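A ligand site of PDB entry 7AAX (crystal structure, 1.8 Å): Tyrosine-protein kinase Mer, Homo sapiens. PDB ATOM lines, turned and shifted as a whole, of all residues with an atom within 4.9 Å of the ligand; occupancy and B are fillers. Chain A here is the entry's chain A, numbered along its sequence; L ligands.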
ATOM      1  N   LEU A  27     -11.555  -0.254  29.207  1.00  0.00           N
ATOM      2  CA  LEU A  27     -12.909  -0.711  29.444  1.00  0.00           C
ATOM      3  C   LEU A  27     -12.977  -1.638  30.671  1.00  0.00           C
ATOM      4  O   LEU A  27     -14.022  -1.765  31.274  1.00  0.00           O
ATOM      5  CB  LEU A  27     -13.435  -1.445  28.217  1.00  0.00           C
ATOM      6  CG  LEU A  27     -13.471  -0.698  26.879  1.00  0.00           C
ATOM      7  CD1 LEU A  27     -13.601  -1.688  25.735  1.00  0.00           C
ATOM      8  CD2 LEU A  27     -14.613   0.299  26.818  1.00  0.00           C
ATOM      9  N   GLY A  28     -11.885  -2.302  31.022  1.00  0.00           N
ATOM     10  CA  GLY A  28     -11.871  -3.239  32.145  1.00  0.00           C
ATOM     11  C   GLY A  28     -10.447  -3.633  32.497  1.00  0.00           C
ATOM     12  O   GLY A  28      -9.593  -3.729  31.626  1.00  0.00           O
ATOM     13  N   VAL A  35      -8.909  -4.862  29.143  1.00  0.00           N
ATOM     14  CA  VAL A  35      -9.613  -4.710  27.894  1.00  0.00           C
ATOM     15  C   VAL A  35      -9.628  -3.215  27.638  1.00  0.00           C
ATOM     16  O   VAL A  35      -9.961  -2.430  28.545  1.00  0.00           O
ATOM     17  CB  VAL A  35     -11.069  -5.239  27.971  1.00  0.00           C
ATOM     18  CG1 VAL A  35     -11.790  -5.101  26.626  1.00  0.00           C
ATOM     19  CG2 VAL A  35     -11.072  -6.672  28.430  1.00  0.00           C
ATOM     20  N   ALA A  51     -12.404  -3.968  20.417  1.00  0.00           N
ATOM     21  CA  ALA A  51     -11.961  -4.166  21.773  1.00  0.00           C
ATOM     22  C   ALA A  51     -10.696  -5.009  21.685  1.00  0.00           C
ATOM     23  O   ALA A  51     -10.592  -5.887  20.852  1.00  0.00           O
ATOM     24  CB  ALA A  51     -13.015  -4.873  22.603  1.00  0.00           C
ATOM     25  N   VAL A  52      -9.760  -4.750  22.602  1.00  0.00           N
ATOM     26  CA  VAL A  52      -8.453  -5.409  22.625  1.00  0.00           C
ATOM     27  C   VAL A  52      -8.196  -5.898  24.044  1.00  0.00           C
ATOM     28  O   VAL A  52      -8.128  -5.073  24.976  1.00  0.00           O
ATOM     29  CB  VAL A  52      -7.317  -4.435  22.243  1.00  0.00           C
ATOM     30  CG1 VAL A  52      -5.971  -5.154  22.168  1.00  0.00           C
ATOM     31  CG2 VAL A  52      -7.654  -3.694  20.954  1.00  0.00           C
ATOM     32  N   LYS A  53      -8.101  -7.209  24.208  1.00  0.00           N
ATOM     33  CA  LYS A  53      -7.828  -7.786  25.526  1.00  0.00           C
ATOM     34  C   LYS A  53      -6.359  -8.071  25.573  1.00  0.00           C
ATOM     35  O   LYS A  53      -5.866  -8.733  24.695  1.00  0.00           O
ATOM     36  CB  LYS A  53      -8.607  -9.076  25.725  1.00  0.00           C
ATOM     37  CG  LYS A  53      -8.517  -9.604  27.155  1.00  0.00           C
ATOM     38  CD  LYS A  53      -8.877 -11.076  27.225  1.00  0.00           C
ATOM     39  CE  LYS A  53      -8.733 -11.625  28.636  1.00  0.00           C
ATOM     40  NZ  LYS A  53      -9.602 -10.908  29.638  1.00  0.00           N
ATOM     41  N   PHE A  68      -1.011 -19.817  22.777  1.00  0.00           N
ATOM     42  CA  PHE A  68      -1.920 -18.699  22.608  1.00  0.00           C
ATOM     43  C   PHE A  68      -2.223 -18.469  21.122  1.00  0.00           C
ATOM     44  O   PHE A  68      -3.388 -18.340  20.739  1.00  0.00           O
ATOM     45  CB  PHE A  68      -1.352 -17.446  23.279  1.00  0.00           C
ATOM     46  CG  PHE A  68      -2.024 -16.169  22.902  1.00  0.00           C
ATOM     47  CD1 PHE A  68      -3.169 -15.740  23.560  1.00  0.00           C
ATOM     48  CD2 PHE A  68      -1.521 -15.379  21.875  1.00  0.00           C
ATOM     49  CE1 PHE A  68      -3.809 -14.572  23.190  1.00  0.00           C
ATOM     50  CE2 PHE A  68      -2.177 -14.205  21.490  1.00  0.00           C
ATOM     51  CZ  PHE A  68      -3.317 -13.799  22.154  1.00  0.00           C
ATOM     52  N   GLU A  71      -4.312 -21.435  19.694  1.00  0.00           N
ATOM     53  CA  GLU A  71      -5.689 -21.320  20.167  1.00  0.00           C
ATOM     54  C   GLU A  71      -6.427 -20.215  19.446  1.00  0.00           C
ATOM     55  O   GLU A  71      -7.561 -20.402  18.988  1.00  0.00           O
ATOM     56  CB  GLU A  71      -5.750 -21.080  21.696  1.00  0.00           C
ATOM     57  CG  GLU A  71      -5.584 -22.342  22.544  1.00  0.00           C
ATOM     58  CD  GLU A  71      -6.823 -23.248  22.594  1.00  0.00           C
ATOM     59  OE1 GLU A  71      -7.974 -22.738  22.566  1.00  0.00           O
ATOM     60  OE2 GLU A  71      -6.639 -24.493  22.674  1.00  0.00           O
ATOM     61  N   ALA A  72      -5.788 -19.063  19.350  1.00  0.00           N
ATOM     62  CA  ALA A  72      -6.332 -17.919  18.606  1.00  0.00           C
ATOM     63  C   ALA A  72      -6.633 -18.254  17.172  1.00  0.00           C
ATOM     64  O   ALA A  72      -7.666 -17.850  16.650  1.00  0.00           O
ATOM     65  CB  ALA A  72      -5.351 -16.754  18.650  1.00  0.00           C
ATOM     66  N   MET A  75      -9.902 -20.158  17.038  1.00  0.00           N
ATOM     67  CA  MET A  75     -11.076 -19.278  17.306  1.00  0.00           C
ATOM     68  C   MET A  75     -11.411 -18.444  16.061  1.00  0.00           C
ATOM     69  O   MET A  75     -12.570 -18.356  15.671  1.00  0.00           O
ATOM     70  CB  MET A  75     -10.842 -18.287  18.452  1.00  0.00           C
ATOM     71  CG  MET A  75     -10.325 -18.802  19.802  1.00  0.00           C
ATOM     72  SD  MET A  75     -11.225 -20.120  20.646  1.00  0.00           S
ATOM     73  CE  MET A  75     -10.103 -20.405  22.015  1.00  0.00           C
ATOM     74  N   ILE A  84     -18.490 -15.133  18.891  1.00  0.00           N
ATOM     75  CA  ILE A  84     -17.782 -13.879  18.658  1.00  0.00           C
ATOM     76  C   ILE A  84     -16.759 -14.062  17.553  1.00  0.00           C
ATOM     77  O   ILE A  84     -16.190 -15.134  17.436  1.00  0.00           O
ATOM     78  CB  ILE A  84     -17.139 -13.348  19.941  1.00  0.00           C
ATOM     79  CG1 ILE A  84     -16.693 -11.893  19.712  1.00  0.00           C
ATOM     80  CG2 ILE A  84     -15.990 -14.243  20.396  1.00  0.00           C
ATOM     81  CD1 ILE A  84     -16.480 -11.111  20.986  1.00  0.00           C
ATOM     82  N   LEU A  86     -13.168 -13.407  16.190  1.00  0.00           N
ATOM     83  CA  LEU A  86     -11.837 -12.921  16.548  1.00  0.00           C
ATOM     84  C   LEU A  86     -11.232 -12.342  15.266  1.00  0.00           C
ATOM     85  O   LEU A  86     -11.106 -13.029  14.259  1.00  0.00           O
ATOM     86  CB  LEU A  86     -11.017 -14.083  17.066  1.00  0.00           C
ATOM     87  CG  LEU A  86      -9.626 -13.761  17.589  1.00  0.00           C
ATOM     88  CD1 LEU A  86      -9.304 -14.731  18.689  1.00  0.00           C
ATOM     89  CD2 LEU A  86      -8.562 -13.895  16.520  1.00  0.00           C
ATOM     90  N   VAL A 103      -5.633  -9.787  22.036  1.00  0.00           N
ATOM     91  CA  VAL A 103      -6.680 -10.368  21.233  1.00  0.00           C
ATOM     92  C   VAL A 103      -7.613  -9.220  20.770  1.00  0.00           C
ATOM     93  O   VAL A 103      -8.055  -8.422  21.589  1.00  0.00           O
ATOM     94  CB  VAL A 103      -7.443 -11.422  22.056  1.00  0.00           C
ATOM     95  CG1 VAL A 103      -8.639 -11.972  21.308  1.00  0.00           C
ATOM     96  CG2 VAL A 103      -6.519 -12.578  22.438  1.00  0.00           C
ATOM     97  N   LEU A 105     -11.095  -7.985  18.931  1.00  0.00           N
ATOM     98  CA  LEU A 105     -12.459  -8.363  18.566  1.00  0.00           C
ATOM     99  C   LEU A 105     -13.265  -7.127  18.156  1.00  0.00           C
ATOM    100  O   LEU A 105     -12.930  -6.047  18.547  1.00  0.00           O
ATOM    101  CB  LEU A 105     -13.110  -8.987  19.800  1.00  0.00           C
ATOM    102  CG  LEU A 105     -12.267 -10.175  20.331  1.00  0.00           C
ATOM    103  CD1 LEU A 105     -11.343  -9.726  21.473  1.00  0.00           C
ATOM    104  CD2 LEU A 105     -13.107 -11.340  20.778  1.00  0.00           C
ATOM    105  N   PRO A 106     -14.360  -7.281  17.406  1.00  0.00           N
ATOM    106  CA  PRO A 106     -15.207  -6.118  17.127  1.00  0.00           C
ATOM    107  C   PRO A 106     -15.784  -5.529  18.424  1.00  0.00           C
ATOM    108  O   PRO A 106     -16.018  -6.258  19.362  1.00  0.00           O
ATOM    109  CB  PRO A 106     -16.335  -6.690  16.244  1.00  0.00           C
ATOM    110  CG  PRO A 106     -15.888  -8.055  15.865  1.00  0.00           C
ATOM    111  CD  PRO A 106     -15.009  -8.520  16.980  1.00  0.00           C
ATOM    112  N   PHE A 107     -15.931  -4.226  18.500  1.00  0.00           N
ATOM    113  CA  PHE A 107     -16.329  -3.573  19.732  1.00  0.00           C
ATOM    114  C   PHE A 107     -17.833  -3.694  19.815  1.00  0.00           C
ATOM    115  O   PHE A 107     -18.529  -3.415  18.825  1.00  0.00           O
ATOM    116  CB  PHE A 107     -15.912  -2.118  19.742  1.00  0.00           C
ATOM    117  CG  PHE A 107     -16.424  -1.322  20.905  1.00  0.00           C
ATOM    118  CD1 PHE A 107     -15.773  -1.346  22.124  1.00  0.00           C
ATOM    119  CD2 PHE A 107     -17.524  -0.483  20.756  1.00  0.00           C
ATOM    120  CE1 PHE A 107     -16.220  -0.600  23.178  1.00  0.00           C
ATOM    121  CE2 PHE A 107     -17.978   0.284  21.813  1.00  0.00           C
ATOM    122  CZ  PHE A 107     -17.337   0.227  23.042  1.00  0.00           C
ATOM    123  N   MET A 108     -18.336  -4.153  20.964  1.00  0.00           N
ATOM    124  CA  MET A 108     -19.779  -4.298  21.115  1.00  0.00           C
ATOM    125  C   MET A 108     -20.249  -3.400  22.230  1.00  0.00           C
ATOM    126  O   MET A 108     -19.972  -3.656  23.397  1.00  0.00           O
ATOM    127  CB  MET A 108     -20.120  -5.743  21.350  1.00  0.00           C
ATOM    128  CG  MET A 108     -20.021  -6.536  20.049  1.00  0.00           C
ATOM    129  SD  MET A 108     -20.194  -8.299  20.286  1.00  0.00           S
ATOM    130  CE  MET A 108     -18.728  -8.650  21.236  1.00  0.00           C
ATOM    131  N   LYS A 109     -20.919  -2.308  21.842  1.00  0.00           N
ATOM    132  CA  LYS A 109     -21.204  -1.201  22.777  1.00  0.00           C
ATOM    133  C   LYS A 109     -22.073  -1.637  23.927  1.00  0.00           C
ATOM    134  O   LYS A 109     -21.916  -1.125  25.021  1.00  0.00           O
ATOM    135  CB  LYS A 109     -21.836   0.011  22.084  1.00  0.00           C
ATOM    136  CG  LYS A 109     -23.209  -0.209  21.484  1.00  0.00           C
ATOM    137  CD  LYS A 109     -23.579   0.977  20.603  1.00  0.00           C
ATOM    138  CE  LYS A 109     -25.042   0.976  20.263  1.00  0.00           C
ATOM    139  NZ  LYS A 109     -25.337   2.176  19.421  1.00  0.00           N
ATOM    140  N   GLY A 111     -21.962  -4.448  25.450  1.00  0.00           N
ATOM    141  CA  GLY A 111     -21.157  -5.105  26.494  1.00  0.00           C
ATOM    142  C   GLY A 111     -21.651  -6.542  26.788  1.00  0.00           C
ATOM    143  O   GLY A 111     -22.343  -7.163  25.975  1.00  0.00           O
ATOM    144  N   PHE A 153     -15.629 -28.404  20.120  1.00  0.00           N
ATOM    145  CA  PHE A 153     -14.972 -27.418  20.942  1.00  0.00           C
ATOM    146  C   PHE A 153     -15.683 -27.445  22.297  1.00  0.00           C
ATOM    147  O   PHE A 153     -16.909 -27.435  22.375  1.00  0.00           O
ATOM    148  CB  PHE A 153     -15.027 -26.042  20.288  1.00  0.00           C
ATOM    149  CG  PHE A 153     -14.394 -24.958  21.104  1.00  0.00           C
ATOM    150  CD1 PHE A 153     -13.006 -24.756  21.067  1.00  0.00           C
ATOM    151  CD2 PHE A 153     -15.167 -24.127  21.917  1.00  0.00           C
ATOM    152  CE1 PHE A 153     -12.413 -23.757  21.828  1.00  0.00           C
ATOM    153  CE2 PHE A 153     -14.573 -23.119  22.680  1.00  0.00           C
ATOM    154  CZ  PHE A 153     -13.196 -22.934  22.636  1.00  0.00           C
ATOM    155  N   HIS A 155     -16.231 -25.375  25.654  1.00  0.00           N
ATOM    156  CA  HIS A 155     -16.144 -24.002  26.127  1.00  0.00           C
ATOM    157  C   HIS A 155     -15.459 -23.891  27.487  1.00  0.00           C
ATOM    158  O   HIS A 155     -14.468 -23.180  27.589  1.00  0.00           O
ATOM    159  CB  HIS A 155     -17.540 -23.375  26.175  1.00  0.00           C
ATOM    160  CG  HIS A 155     -17.531 -21.891  26.260  1.00  0.00           C
ATOM    161  ND1 HIS A 155     -17.051 -21.213  27.360  1.00  0.00           N
ATOM    162  CD2 HIS A 155     -17.972 -20.955  25.404  1.00  0.00           C
ATOM    163  CE1 HIS A 155     -17.167 -19.910  27.155  1.00  0.00           C
ATOM    164  NE2 HIS A 155     -17.744 -19.739  25.985  1.00  0.00           N
ATOM    165  N   MET A 164     -21.840 -11.904  24.792  1.00  0.00           N
ATOM    166  CA  MET A 164     -21.796 -10.499  24.426  1.00  0.00           C
ATOM    167  C   MET A 164     -22.999 -10.143  23.555  1.00  0.00           C
ATOM    168  O   MET A 164     -23.494 -10.968  22.815  1.00  0.00           O
ATOM    169  CB  MET A 164     -20.506 -10.207  23.664  1.00  0.00           C
ATOM    170  CG  MET A 164     -19.257 -10.459  24.478  1.00  0.00           C
ATOM    171  SD  MET A 164     -18.970  -9.283  25.805  1.00  0.00           S
ATOM    172  CE  MET A 164     -18.853  -7.744  24.912  1.00  0.00           C
ATOM    173  N   VAL A 173     -21.594 -16.044  21.892  1.00  0.00           N
ATOM    174  CA  VAL A 173     -20.732 -16.740  22.827  1.00  0.00           C
ATOM    175  C   VAL A 173     -19.298 -16.201  22.723  1.00  0.00           C
ATOM    176  O   VAL A 173     -18.768 -16.067  21.614  1.00  0.00           O
ATOM    177  CB  VAL A 173     -20.797 -18.251  22.555  1.00  0.00           C
ATOM    178  CG1 VAL A 173     -19.843 -19.011  23.463  1.00  0.00           C
ATOM    179  CG2 VAL A 173     -22.243 -18.716  22.813  1.00  0.00           C
ATOM    180  N   ALA A 174     -18.718 -15.881  23.881  1.00  0.00           N
ATOM    181  CA  ALA A 174     -17.326 -15.396  24.031  1.00  0.00           C
ATOM    182  C   ALA A 174     -16.622 -16.029  25.253  1.00  0.00           C
ATOM    183  O   ALA A 174     -17.133 -16.984  25.850  1.00  0.00           O
ATOM    184  CB  ALA A 174     -17.356 -13.898  24.117  1.00  0.00           C
ATOM    185  N   ASP A 175     -15.471 -15.501  25.635  1.00  0.00           N
ATOM    186  CA  ASP A 175     -14.717 -16.035  26.779  1.00  0.00           C
ATOM    187  C   ASP A 175     -13.642 -15.014  27.209  1.00  0.00           C
ATOM    188  O   ASP A 175     -12.650 -14.849  26.522  1.00  0.00           O
ATOM    189  CB  ASP A 175     -14.096 -17.392  26.351  1.00  0.00           C
ATOM    190  CG  ASP A 175     -13.556 -18.204  27.519  1.00  0.00           C
ATOM    191  OD1 ASP A 175     -13.346 -17.668  28.625  1.00  0.00           O
ATOM    192  OD2 ASP A 175     -13.342 -19.413  27.304  1.00  0.00           O
ATOM    193  N   PHE A 176     -13.869 -14.313  28.316  1.00  0.00           N
ATOM    194  CA  PHE A 176     -12.915 -13.311  28.820  1.00  0.00           C
ATOM    195  C   PHE A 176     -11.609 -13.924  29.373  1.00  0.00           C
ATOM    196  O   PHE A 176     -11.530 -15.138  29.684  1.00  0.00           O
ATOM    197  CB  PHE A 176     -13.583 -12.413  29.890  1.00  0.00           C
ATOM    198  CG  PHE A 176     -14.472 -11.314  29.322  1.00  0.00           C
ATOM    199  CD1 PHE A 176     -15.809 -11.574  28.973  1.00  0.00           C
ATOM    200  CD2 PHE A 176     -13.989 -10.008  29.167  1.00  0.00           C
ATOM    201  CE1 PHE A 176     -16.641 -10.563  28.479  1.00  0.00           C
ATOM    202  CE2 PHE A 176     -14.820  -8.987  28.676  1.00  0.00           C
ATOM    203  CZ  PHE A 176     -16.149  -9.268  28.325  1.00  0.00           C
HETATM  204  C1  LIG L   1     -14.159 -18.347  22.925  1.00  0.00           C
HETATM  205  C2  LIG L   1     -12.625 -16.440  23.071  1.00  0.00           C
HETATM  206  C3  LIG L   1     -11.483 -17.197  23.091  1.00  0.00           C
HETATM  207  O1  LIG L   1     -16.200  -4.035  28.371  1.00  0.00           O
HETATM  208  C4  LIG L   1     -14.279 -11.393  24.751  1.00  0.00           C
HETATM  209  C5  LIG L   1     -14.795 -10.154  25.077  1.00  0.00           C
HETATM  210  C6  LIG L   1     -13.946  -9.070  25.198  1.00  0.00           C
HETATM  211  C7  LIG L   1     -15.133  -7.042  24.642  1.00  0.00           C
HETATM  212  C8  LIG L   1     -15.318  -7.323  23.313  1.00  0.00           C
HETATM  213  C9  LIG L   1     -16.125  -6.467  22.575  1.00  0.00           C
HETATM  214  C10 LIG L   1     -16.571  -5.111  24.379  1.00  0.00           C
HETATM  215  C11 LIG L   1     -17.218  -3.976  24.907  1.00  0.00           C
HETATM  216  C12 LIG L   1     -17.068  -3.660  26.232  1.00  0.00           C
HETATM  217  C13 LIG L   1     -18.665  -1.855  26.146  1.00  0.00           C
HETATM  218  C14 LIG L   1     -15.628  -5.562  26.579  1.00  0.00           C
HETATM  219  C15 LIG L   1     -15.763  -5.911  25.218  1.00  0.00           C
HETATM  220  C16 LIG L   1     -12.605  -9.253  24.988  1.00  0.00           C
HETATM  221  C17 LIG L   1     -12.062 -10.472  24.655  1.00  0.00           C
HETATM  222  C18 LIG L   1      -8.760 -17.537  24.802  1.00  0.00           C
HETATM  223  C19 LIG L   1      -6.844 -16.904  22.903  1.00  0.00           C
HETATM  224  F1  LIG L   1      -5.244 -18.000  24.219  1.00  0.00           F
HETATM  225  C20 LIG L   1      -6.527 -17.611  24.031  1.00  0.00           C
HETATM  226  C21 LIG L   1      -7.449 -17.930  24.998  1.00  0.00           C
HETATM  227  C22 LIG L   1      -8.157 -16.486  22.691  1.00  0.00           C
HETATM  228  C23 LIG L   1      -8.496 -15.718  21.462  1.00  0.00           C
HETATM  229  C24 LIG L   1      -9.091 -16.815  23.661  1.00  0.00           C
HETATM  230  N1  LIG L   1     -10.456 -16.426  23.500  1.00  0.00           N
HETATM  231  N2  LIG L   1     -10.854 -15.150  23.767  1.00  0.00           N
HETATM  232  C25 LIG L   1     -12.172 -15.145  23.509  1.00  0.00           C
HETATM  233  O2  LIG L   1     -13.855 -16.921  22.695  1.00  0.00           O
HETATM  234  C26 LIG L   1     -15.646 -18.619  22.826  1.00  0.00           C
HETATM  235  C27 LIG L   1     -12.996 -13.929  23.683  1.00  0.00           C
HETATM  236  O3  LIG L   1     -14.197 -13.952  23.371  1.00  0.00           O
HETATM  237  N3  LIG L   1     -12.343 -12.819  24.198  1.00  0.00           N
HETATM  238  C28 LIG L   1     -12.912 -11.566  24.531  1.00  0.00           C
HETATM  239  F2  LIG L   1     -11.789  -8.186  25.105  1.00  0.00           F
HETATM  240  O4  LIG L   1     -14.359  -7.779  25.528  1.00  0.00           O
HETATM  241  N4  LIG L   1     -16.746  -5.393  23.053  1.00  0.00           N
HETATM  242  C29 LIG L   1     -16.269  -4.459  27.068  1.00  0.00           C
HETATM  243  C30 LIG L   1     -15.285  -4.718  29.241  1.00  0.00           C
HETATM  244  O5  LIG L   1     -17.648  -2.588  26.854  1.00  0.00           O
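Residues that only touch the ligand: Leu 27 (3.8 Å), Val 35 (3.4 Å), Ala 51 (3.4 Å), Lys 53 (3.4 Å), Phe 68 (3.1 Å), Met 75 (3.7 Å), Ile 84 (3.5 Å), Leu 86 (3.1 Å), Val 103 (3.8 Å), Leu 105 (3.3 Å), Pro 106 (3.2 Å), Phe 107 (3.8 Å), Lys 109 (3.5 Å), His 155 (3.95 Å), Met 164 (3.5 Å), Ala 174 (3.2 Å) and Phe 176 (3.4 Å). Hydrophobic or aromatic side chains that line the ligand: Leu 27, Val 35, Ala 51, Phe 68, Met 75, Ile 84, Leu 86, Val 103, Leu 105, Phe 107, Met 108, Met 164, Ala 174 and Phe 176. 19 residues have an atom within 4 Å of the ligand: Leu 27, Val 35, Ala 51, Lys 53, Phe 68, Met 75, Ile 84, Leu 86, Val 103, Leu 105, Pro 106, Phe 107, Met 108, Lys 109, His 155, Met 164, Ala 174, Asp 175 and Phe 176.
The backbone NH of Ile 84 is in hydrogen-bond range of the backbone carbonyl oxygen of Val 173. N of Val 103 is in hydrogen-bond range of O of Lys 53, 2.9 Å away. The backbone NH (N) of Val 35 sits at hydrogen-bond distance from the backbone carbonyl oxygen (O) of Gly 28. A ring nitrogen (NE2) of His 155 sits at hydrogen-bond distance from the backbone carbonyl oxygen (O) of Ala 174 (2.8 Å). The backbone carbonyl oxygen (O) of Leu 105 lies within hydrogen-bond range of the backbone NH (N) of Ala 51 (2.8 Å). O of Val 35 lies within hydrogen-bond range of N of Leu 27 (2.8 Å).
A nitrogen (N3) of the ligand sits close to the backbone carbonyl oxygen (O) of Asp 175. An oxygen (O3) of the ligand sits at hydrogen-bond distance from the backbone NH (N) of Asp 175 (3.0 Å). N of Met 108 sits at hydrogen-bond distance from N4 of the ligand, 2.9 Å away.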
